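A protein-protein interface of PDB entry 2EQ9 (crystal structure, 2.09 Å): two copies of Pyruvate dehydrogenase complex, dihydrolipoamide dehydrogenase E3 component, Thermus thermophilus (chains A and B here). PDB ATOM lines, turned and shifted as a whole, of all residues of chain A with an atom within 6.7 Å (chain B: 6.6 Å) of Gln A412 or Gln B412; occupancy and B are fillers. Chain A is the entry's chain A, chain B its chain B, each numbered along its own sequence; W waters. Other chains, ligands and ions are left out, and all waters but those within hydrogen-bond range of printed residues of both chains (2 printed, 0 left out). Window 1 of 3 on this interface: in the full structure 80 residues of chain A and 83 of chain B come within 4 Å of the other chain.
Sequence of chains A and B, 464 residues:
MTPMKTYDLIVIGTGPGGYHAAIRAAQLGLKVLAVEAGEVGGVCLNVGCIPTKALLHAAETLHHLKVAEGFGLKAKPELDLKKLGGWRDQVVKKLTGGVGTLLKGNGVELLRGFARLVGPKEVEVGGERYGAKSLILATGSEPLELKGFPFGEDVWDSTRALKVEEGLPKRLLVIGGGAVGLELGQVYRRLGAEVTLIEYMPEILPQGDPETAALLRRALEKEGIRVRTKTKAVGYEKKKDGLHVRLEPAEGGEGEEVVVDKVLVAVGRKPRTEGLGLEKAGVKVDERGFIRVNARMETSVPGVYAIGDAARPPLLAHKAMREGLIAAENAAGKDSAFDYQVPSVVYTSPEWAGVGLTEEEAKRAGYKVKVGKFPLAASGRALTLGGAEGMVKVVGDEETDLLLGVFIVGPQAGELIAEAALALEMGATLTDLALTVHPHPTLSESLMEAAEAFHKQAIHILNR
Gln A412 touches just one residue of chain B: Gln B412 (3.6 Å). Printed residues of chain B within 4 Å of Glu A415: Leu B416 (3.4 Å) and Leu B443 (2.8 Å). Pro B350 touches none of the printed residues of chain A. Gln B412 touches just one residue of chain A: Gln A412 (3.6 Å). Of the printed residues of chain A, Leu B416 touches Glu A415. Of the printed residues of chain A, Leu B443 touches Glu A415 (2.8 Å).
Gln A412 touches Gln B412 (OE1 to OE1, 3.6 Å). CD2 of Leu B416 touches OE2 of Glu A415, at 3.4 Å. CD2 of Leu A416 touches OE2 of Glu B415, at 3.5 Å.
The backbone NH of Leu A443 lies within hydrogen-bond range of the side-chain carboxylate of Glu B415, 2.7 Å away. OE1 of Glu A415 is in hydrogen-bond range of N of Leu B443 (2.8 Å).
Gln A412 touches its own counterpart, Gln B412. Glu A415 touches Leu B416, and with the chains exchanged Leu A416 touches Glu B415. Glu A415 touches Leu B443, and with the chains exchanged Leu A443 touches Glu B415. Positions printed for both chains: 350, 351, 353, 381, 385, 408, 410, 411, 412, 413, 414, 415, 416, 417 and 443. Of the 5 pairs that touch across the chains among the printed residues, 5 have their exchanged pair printed and touching as well.
Water W2 lies within hydrogen-bond range of the guanidinium group of Arg A381 and the side-chain carboxylate of Glu B351. Water W1 bridges OE2 of Glu A351 (2.6 Å) and NH2 of Arg B381 (3.5 Å).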
ATOM      1  N   PRO A 350      28.073 -30.758 -34.214  1.00  0.00           N
ATOM      2  CA  PRO A 350      27.898 -29.553 -33.399  1.00  0.00           C
ATOM      3  C   PRO A 350      26.449 -29.173 -33.111  1.00  0.00           C
ATOM      4  O   PRO A 350      25.540 -29.512 -33.862  1.00  0.00           O
ATOM      5  CB  PRO A 350      28.593 -28.487 -34.229  1.00  0.00           C
ATOM      6  CG  PRO A 350      28.240 -28.910 -35.633  1.00  0.00           C
ATOM      7  CD  PRO A 350      28.506 -30.404 -35.580  1.00  0.00           C
ATOM      8  N   GLU A 351      26.249 -28.461 -32.008  1.00  0.00           N
ATOM      9  CA  GLU A 351      24.928 -27.983 -31.622  1.00  0.00           C
ATOM     10  C   GLU A 351      24.579 -26.754 -32.463  1.00  0.00           C
ATOM     11  O   GLU A 351      25.460 -26.099 -33.028  1.00  0.00           O
ATOM     12  CB  GLU A 351      24.911 -27.586 -30.142  1.00  0.00           C
ATOM     13  CG  GLU A 351      24.749 -28.741 -29.166  1.00  0.00           C
ATOM     14  CD  GLU A 351      24.825 -28.292 -27.714  1.00  0.00           C
ATOM     15  OE1 GLU A 351      24.415 -27.145 -27.409  1.00  0.00           O
ATOM     16  OE2 GLU A 351      25.289 -29.095 -26.878  1.00  0.00           O
ATOM     17  N   ALA A 353      21.936 -23.258 -32.354  1.00  0.00           N
ATOM     18  CA  ALA A 353      21.068 -22.474 -31.495  1.00  0.00           C
ATOM     19  C   ALA A 353      20.798 -21.142 -32.176  1.00  0.00           C
ATOM     20  O   ALA A 353      21.629 -20.640 -32.936  1.00  0.00           O
ATOM     21  CB  ALA A 353      21.734 -22.257 -30.157  1.00  0.00           C
ATOM     22  N   ARG A 381      39.963 -21.748 -27.553  1.00  0.00           N
ATOM     23  CA  ARG A 381      39.290 -22.737 -26.722  1.00  0.00           C
ATOM     24  C   ARG A 381      38.842 -23.940 -27.536  1.00  0.00           C
ATOM     25  O   ARG A 381      38.951 -25.077 -27.085  1.00  0.00           O
ATOM     26  CB  ARG A 381      38.065 -22.118 -26.040  1.00  0.00           C
ATOM     27  CG  ARG A 381      37.312 -23.078 -25.115  1.00  0.00           C
ATOM     28  CD  ARG A 381      38.279 -23.744 -24.144  1.00  0.00           C
ATOM     29  NE  ARG A 381      37.616 -24.416 -23.032  1.00  0.00           N
ATOM     30  CZ  ARG A 381      38.091 -25.499 -22.426  1.00  0.00           C
ATOM     31  NH1 ARG A 381      39.236 -26.043 -22.824  1.00  0.00           N
ATOM     32  NH2 ARG A 381      37.422 -26.043 -21.419  1.00  0.00           N
ATOM     33  N   LEU A 385      39.918 -28.099 -27.261  1.00  0.00           N
ATOM     34  CA  LEU A 385      38.868 -29.105 -27.125  1.00  0.00           C
ATOM     35  C   LEU A 385      38.919 -30.097 -28.282  1.00  0.00           C
ATOM     36  O   LEU A 385      38.094 -31.010 -28.366  1.00  0.00           O
ATOM     37  CB  LEU A 385      37.490 -28.439 -27.103  1.00  0.00           C
ATOM     38  CG  LEU A 385      37.188 -27.506 -25.930  1.00  0.00           C
ATOM     39  CD1 LEU A 385      35.799 -26.903 -26.107  1.00  0.00           C
ATOM     40  CD2 LEU A 385      37.284 -28.279 -24.618  1.00  0.00           C
ATOM     41  N   ILE A 408      24.117 -19.624 -33.707  1.00  0.00           N
ATOM     42  CA  ILE A 408      25.371 -20.287 -33.390  1.00  0.00           C
ATOM     43  C   ILE A 408      25.359 -21.769 -33.733  1.00  0.00           C
ATOM     44  O   ILE A 408      24.365 -22.458 -33.522  1.00  0.00           O
ATOM     45  CB  ILE A 408      25.658 -20.170 -31.876  1.00  0.00           C
ATOM     46  CG1 ILE A 408      25.478 -18.712 -31.428  1.00  0.00           C
ATOM     47  CG2 ILE A 408      27.068 -20.689 -31.561  1.00  0.00           C
ATOM     48  CD1 ILE A 408      25.322 -18.533 -29.925  1.00  0.00           C
ATOM     49  N   GLY A 410      28.088 -24.987 -33.161  1.00  0.00           N
ATOM     50  CA  GLY A 410      29.359 -25.377 -32.580  1.00  0.00           C
ATOM     51  C   GLY A 410      29.142 -26.027 -31.227  1.00  0.00           C
ATOM     52  O   GLY A 410      28.000 -26.160 -30.788  1.00  0.00           O
ATOM     53  N   PRO A 411      30.206 -26.447 -30.532  1.00  0.00           N
ATOM     54  CA  PRO A 411      29.966 -27.070 -29.233  1.00  0.00           C
ATOM     55  C   PRO A 411      29.418 -26.072 -28.221  1.00  0.00           C
ATOM     56  O   PRO A 411      29.811 -24.908 -28.208  1.00  0.00           O
ATOM     57  CB  PRO A 411      31.341 -27.611 -28.850  1.00  0.00           C
ATOM     58  CG  PRO A 411      32.276 -26.667 -29.524  1.00  0.00           C
ATOM     59  CD  PRO A 411      31.637 -26.469 -30.874  1.00  0.00           C
ATOM     60  N   GLN A 412      28.483 -26.534 -27.398  1.00  0.00           N
ATOM     61  CA  GLN A 412      27.880 -25.699 -26.368  1.00  0.00           C
ATOM     62  C   GLN A 412      27.043 -24.542 -26.914  1.00  0.00           C
ATOM     63  O   GLN A 412      26.740 -23.602 -26.182  1.00  0.00           O
ATOM     64  CB  GLN A 412      28.973 -25.166 -25.444  1.00  0.00           C
ATOM     65  CG  GLN A 412      29.924 -26.262 -24.947  1.00  0.00           C
ATOM     66  CD  GLN A 412      29.194 -27.382 -24.217  1.00  0.00           C
ATOM     67  OE1 GLN A 412      29.527 -28.559 -24.368  1.00  0.00           O
ATOM     68  NE2 GLN A 412      28.199 -27.018 -23.412  1.00  0.00           N
ATOM     69  N   ALA A 413      26.653 -24.618 -28.186  1.00  0.00           N
ATOM     70  CA  ALA A 413      25.839 -23.563 -28.787  1.00  0.00           C
ATOM     71  C   ALA A 413      24.606 -23.253 -27.949  1.00  0.00           C
ATOM     72  O   ALA A 413      24.208 -22.087 -27.816  1.00  0.00           O
ATOM     73  CB  ALA A 413      25.405 -23.965 -30.196  1.00  0.00           C
ATOM     74  N   GLY A 414      24.003 -24.304 -27.400  1.00  0.00           N
ATOM     75  CA  GLY A 414      22.809 -24.154 -26.595  1.00  0.00           C
ATOM     76  C   GLY A 414      23.014 -23.387 -25.301  1.00  0.00           C
ATOM     77  O   GLY A 414      22.081 -22.755 -24.808  1.00  0.00           O
ATOM     78  N   GLU A 415      24.218 -23.440 -24.740  1.00  0.00           N
ATOM     79  CA  GLU A 415      24.492 -22.721 -23.499  1.00  0.00           C
ATOM     80  C   GLU A 415      24.805 -21.253 -23.793  1.00  0.00           C
ATOM     81  O   GLU A 415      24.444 -20.364 -23.020  1.00  0.00           O
ATOM     82  CB  GLU A 415      25.674 -23.356 -22.765  1.00  0.00           C
ATOM     83  CG  GLU A 415      25.502 -24.840 -22.451  1.00  0.00           C
ATOM     84  CD  GLU A 415      24.444 -25.113 -21.384  1.00  0.00           C
ATOM     85  OE1 GLU A 415      24.085 -26.292 -21.194  1.00  0.00           O
ATOM     86  OE2 GLU A 415      23.978 -24.158 -20.732  1.00  0.00           O
ATOM     87  N   LEU A 416      25.457 -21.005 -24.930  1.00  0.00           N
ATOM     88  CA  LEU A 416      25.837 -19.656 -25.318  1.00  0.00           C
ATOM     89  C   LEU A 416      24.664 -18.818 -25.818  1.00  0.00           C
ATOM     90  O   LEU A 416      24.739 -17.593 -25.824  1.00  0.00           O
ATOM     91  CB  LEU A 416      26.918 -19.704 -26.402  1.00  0.00           C
ATOM     92  CG  LEU A 416      28.142 -20.603 -26.153  1.00  0.00           C
ATOM     93  CD1 LEU A 416      29.098 -20.491 -27.342  1.00  0.00           C
ATOM     94  CD2 LEU A 416      28.850 -20.214 -24.860  1.00  0.00           C
ATOM     95  N   ILE A 417      23.578 -19.472 -26.222  1.00  0.00           N
ATOM     96  CA  ILE A 417      22.426 -18.744 -26.737  1.00  0.00           C
ATOM     97  C   ILE A 417      21.649 -17.996 -25.649  1.00  0.00           C
ATOM     98  O   ILE A 417      20.934 -17.039 -25.940  1.00  0.00           O
ATOM     99  CB  ILE A 417      21.469 -19.685 -27.514  1.00  0.00           C
ATOM    100  CG1 ILE A 417      20.684 -18.879 -28.557  1.00  0.00           C
ATOM    101  CG2 ILE A 417      20.515 -20.389 -26.559  1.00  0.00           C
ATOM    102  CD1 ILE A 417      21.569 -18.245 -29.610  1.00  0.00           C
ATOM    103  N   LEU A 443      34.413 -20.691 -25.302  1.00  0.00           N
ATOM    104  CA  LEU A 443      33.691 -20.675 -26.563  1.00  0.00           C
ATOM    105  C   LEU A 443      32.818 -19.428 -26.625  1.00  0.00           C
ATOM    106  O   LEU A 443      32.588 -18.881 -27.704  1.00  0.00           O
ATOM    107  CB  LEU A 443      32.833 -21.930 -26.695  1.00  0.00           C
ATOM    108  CG  LEU A 443      33.624 -23.247 -26.649  1.00  0.00           C
ATOM    109  CD1 LEU A 443      32.666 -24.428 -26.463  1.00  0.00           C
ATOM    110  CD2 LEU A 443      34.440 -23.411 -27.935  1.00  0.00           C
ATOM    111  N   PRO B 350      34.552 -30.329 -11.495  1.00  0.00           N
ATOM    112  CA  PRO B 350      33.736 -29.274 -12.100  1.00  0.00           C
ATOM    113  C   PRO B 350      34.509 -27.970 -12.245  1.00  0.00           C
ATOM    114  O   PRO B 350      35.541 -27.771 -11.599  1.00  0.00           O
ATOM    115  CB  PRO B 350      32.587 -29.138 -11.113  1.00  0.00           C
ATOM    116  CG  PRO B 350      33.271 -29.369  -9.807  1.00  0.00           C
ATOM    117  CD  PRO B 350      34.112 -30.592 -10.116  1.00  0.00           C
ATOM    118  N   GLU B 351      34.003 -27.090 -13.100  1.00  0.00           N
ATOM    119  CA  GLU B 351      34.621 -25.788 -13.318  1.00  0.00           C
ATOM    120  C   GLU B 351      34.099 -24.801 -12.286  1.00  0.00           C
ATOM    121  O   GLU B 351      33.054 -25.024 -11.671  1.00  0.00           O
ATOM    122  CB  GLU B 351      34.276 -25.255 -14.713  1.00  0.00           C
ATOM    123  CG  GLU B 351      35.058 -25.879 -15.848  1.00  0.00           C
ATOM    124  CD  GLU B 351      34.651 -25.326 -17.209  1.00  0.00           C
ATOM    125  OE1 GLU B 351      34.197 -24.154 -17.280  1.00  0.00           O
ATOM    126  OE2 GLU B 351      34.798 -26.065 -18.207  1.00  0.00           O
ATOM    127  N   ALA B 353      33.518 -20.493 -11.754  1.00  0.00           N
ATOM    128  CA  ALA B 353      33.511 -19.180 -12.393  1.00  0.00           C
ATOM    129  C   ALA B 353      32.847 -18.157 -11.495  1.00  0.00           C
ATOM    130  O   ALA B 353      31.890 -18.466 -10.781  1.00  0.00           O
ATOM    131  CB  ALA B 353      32.777 -19.245 -13.714  1.00  0.00           C
ATOM    132  N   ARG B 381      19.398 -31.211 -17.268  1.00  0.00           N
ATOM    133  CA  ARG B 381      20.510 -31.244 -18.207  1.00  0.00           C
ATOM    134  C   ARG B 381      21.705 -31.912 -17.558  1.00  0.00           C
ATOM    135  O   ARG B 381      22.329 -32.781 -18.152  1.00  0.00           O
ATOM    136  CB  ARG B 381      20.895 -29.826 -18.661  1.00  0.00           C
ATOM    137  CG  ARG B 381      22.048 -29.782 -19.686  1.00  0.00           C
ATOM    138  CD  ARG B 381      21.810 -30.791 -20.809  1.00  0.00           C
ATOM    139  NE  ARG B 381      22.702 -30.629 -21.959  1.00  0.00           N
ATOM    140  CZ  ARG B 381      23.102 -31.636 -22.731  1.00  0.00           C
ATOM    141  NH1 ARG B 381      22.699 -32.874 -22.466  1.00  0.00           N
ATOM    142  NH2 ARG B 381      23.885 -31.410 -23.782  1.00  0.00           N
ATOM    143  N   LEU B 385      23.846 -35.387 -18.550  1.00  0.00           N
ATOM    144  CA  LEU B 385      25.282 -35.336 -18.798  1.00  0.00           C
ATOM    145  C   LEU B 385      26.063 -36.328 -17.932  1.00  0.00           C
ATOM    146  O   LEU B 385      27.295 -36.315 -17.915  1.00  0.00           O
ATOM    147  CB  LEU B 385      25.808 -33.907 -18.592  1.00  0.00           C
ATOM    148  CG  LEU B 385      25.377 -32.897 -19.670  1.00  0.00           C
ATOM    149  CD1 LEU B 385      25.643 -31.465 -19.207  1.00  0.00           C
ATOM    150  CD2 LEU B 385      26.128 -33.198 -20.975  1.00  0.00           C
ATOM    151  N   ILE B 408      29.485 -19.649  -9.970  1.00  0.00           N
ATOM    152  CA  ILE B 408      29.065 -20.959 -10.433  1.00  0.00           C
ATOM    153  C   ILE B 408      30.102 -22.067 -10.261  1.00  0.00           C
ATOM    154  O   ILE B 408      31.301 -21.838 -10.430  1.00  0.00           O
ATOM    155  CB  ILE B 408      28.724 -20.872 -11.930  1.00  0.00           C
ATOM    156  CG1 ILE B 408      27.756 -19.711 -12.161  1.00  0.00           C
ATOM    157  CG2 ILE B 408      28.181 -22.218 -12.431  1.00  0.00           C
ATOM    158  CD1 ILE B 408      27.479 -19.418 -13.620  1.00  0.00           C
ATOM    159  N   GLY B 410      30.396 -26.154 -11.491  1.00  0.00           N
ATOM    160  CA  GLY B 410      29.753 -27.222 -12.226  1.00  0.00           C
ATOM    161  C   GLY B 410      30.302 -27.264 -13.641  1.00  0.00           C
ATOM    162  O   GLY B 410      31.154 -26.448 -14.002  1.00  0.00           O
ATOM    163  N   PRO B 411      29.832 -28.199 -14.476  1.00  0.00           N
ATOM    164  CA  PRO B 411      30.335 -28.277 -15.844  1.00  0.00           C
ATOM    165  C   PRO B 411      29.981 -27.043 -16.663  1.00  0.00           C
ATOM    166  O   PRO B 411      28.884 -26.529 -16.561  1.00  0.00           O
ATOM    167  CB  PRO B 411      29.680 -29.549 -16.370  1.00  0.00           C
ATOM    168  CG  PRO B 411      28.372 -29.566 -15.651  1.00  0.00           C
ATOM    169  CD  PRO B 411      28.748 -29.169 -14.246  1.00  0.00           C
ATOM    170  N   GLN B 412      30.933 -26.546 -17.448  1.00  0.00           N
ATOM    171  CA  GLN B 412      30.686 -25.386 -18.297  1.00  0.00           C
ATOM    172  C   GLN B 412      30.483 -24.061 -17.554  1.00  0.00           C
ATOM    173  O   GLN B 412      29.958 -23.099 -18.118  1.00  0.00           O
ATOM    174  CB  GLN B 412      29.475 -25.669 -19.190  1.00  0.00           C
ATOM    175  CG  GLN B 412      29.594 -26.984 -19.965  1.00  0.00           C
ATOM    176  CD  GLN B 412      30.802 -27.004 -20.889  1.00  0.00           C
ATOM    177  OE1 GLN B 412      31.284 -28.068 -21.270  1.00  0.00           O
ATOM    178  NE2 GLN B 412      31.289 -25.828 -21.260  1.00  0.00           N
ATOM    179  N   ALA B 413      30.896 -24.008 -16.293  1.00  0.00           N
ATOM    180  CA  ALA B 413      30.764 -22.788 -15.503  1.00  0.00           C
ATOM    181  C   ALA B 413      31.403 -21.620 -16.239  1.00  0.00           C
ATOM    182  O   ALA B 413      30.871 -20.509 -16.255  1.00  0.00           O
ATOM    183  CB  ALA B 413      31.439 -22.968 -14.157  1.00  0.00           C
ATOM    184  N   GLY B 414      32.557 -21.887 -16.847  1.00  0.00           N
ATOM    185  CA  GLY B 414      33.270 -20.851 -17.562  1.00  0.00           C
ATOM    186  C   GLY B 414      32.475 -20.267 -18.706  1.00  0.00           C
ATOM    187  O   GLY B 414      32.634 -19.088 -19.032  1.00  0.00           O
ATOM    188  N   GLU B 415      31.616 -21.080 -19.310  1.00  0.00           N
ATOM    189  CA  GLU B 415      30.805 -20.624 -20.435  1.00  0.00           C
ATOM    190  C   GLU B 415      29.578 -19.847 -19.966  1.00  0.00           C
ATOM    191  O   GLU B 415      29.150 -18.892 -20.615  1.00  0.00           O
ATOM    192  CB  GLU B 415      30.360 -21.823 -21.293  1.00  0.00           C
ATOM    193  CG  GLU B 415      31.522 -22.611 -21.925  1.00  0.00           C
ATOM    194  CD  GLU B 415      32.341 -21.780 -22.910  1.00  0.00           C
ATOM    195  OE1 GLU B 415      33.430 -22.233 -23.324  1.00  0.00           O
ATOM    196  OE2 GLU B 415      31.896 -20.671 -23.274  1.00  0.00           O
ATOM    197  N   LEU B 416      29.027 -20.255 -18.829  1.00  0.00           N
ATOM    198  CA  LEU B 416      27.838 -19.628 -18.269  1.00  0.00           C
ATOM    199  C   LEU B 416      28.097 -18.284 -17.601  1.00  0.00           C
ATOM    200  O   LEU B 416      27.183 -17.479 -17.449  1.00  0.00           O
ATOM    201  CB  LEU B 416      27.199 -20.570 -17.254  1.00  0.00           C
ATOM    202  CG  LEU B 416      26.938 -21.994 -17.753  1.00  0.00           C
ATOM    203  CD1 LEU B 416      26.566 -22.893 -16.566  1.00  0.00           C
ATOM    204  CD2 LEU B 416      25.838 -21.983 -18.816  1.00  0.00           C
ATOM    205  N   ILE B 417      29.333 -18.030 -17.194  1.00  0.00           N
ATOM    206  CA  ILE B 417      29.611 -16.772 -16.519  1.00  0.00           C
ATOM    207  C   ILE B 417      29.541 -15.546 -17.428  1.00  0.00           C
ATOM    208  O   ILE B 417      29.358 -14.431 -16.942  1.00  0.00           O
ATOM    209  CB  ILE B 417      30.983 -16.805 -15.815  1.00  0.00           C
ATOM    210  CG1 ILE B 417      30.994 -15.782 -14.680  1.00  0.00           C
ATOM    211  CG2 ILE B 417      32.106 -16.546 -16.811  1.00  0.00           C
ATOM    212  CD1 ILE B 417      30.038 -16.152 -13.558  1.00  0.00           C
ATOM    213  N   LEU B 443      22.366 -26.169 -19.003  1.00  0.00           N
ATOM    214  CA  LEU B 443      22.980 -25.833 -17.737  1.00  0.00           C
ATOM    215  C   LEU B 443      22.704 -24.365 -17.426  1.00  0.00           C
ATOM    216  O   LEU B 443      22.561 -23.982 -16.259  1.00  0.00           O
ATOM    217  CB  LEU B 443      24.486 -26.107 -17.804  1.00  0.00           C
ATOM    218  CG  LEU B 443      24.836 -27.602 -17.914  1.00  0.00           C
ATOM    219  CD1 LEU B 443      26.321 -27.816 -18.205  1.00  0.00           C
ATOM    220  CD2 LEU B 443      24.469 -28.266 -16.611  1.00  0.00           C
HETATM  221  O   HOH W   1      24.718 -31.652 -27.171  1.00  0.00           O
HETATM  222  O   HOH W   2      34.864 -26.057 -20.837  1.00  0.00           O
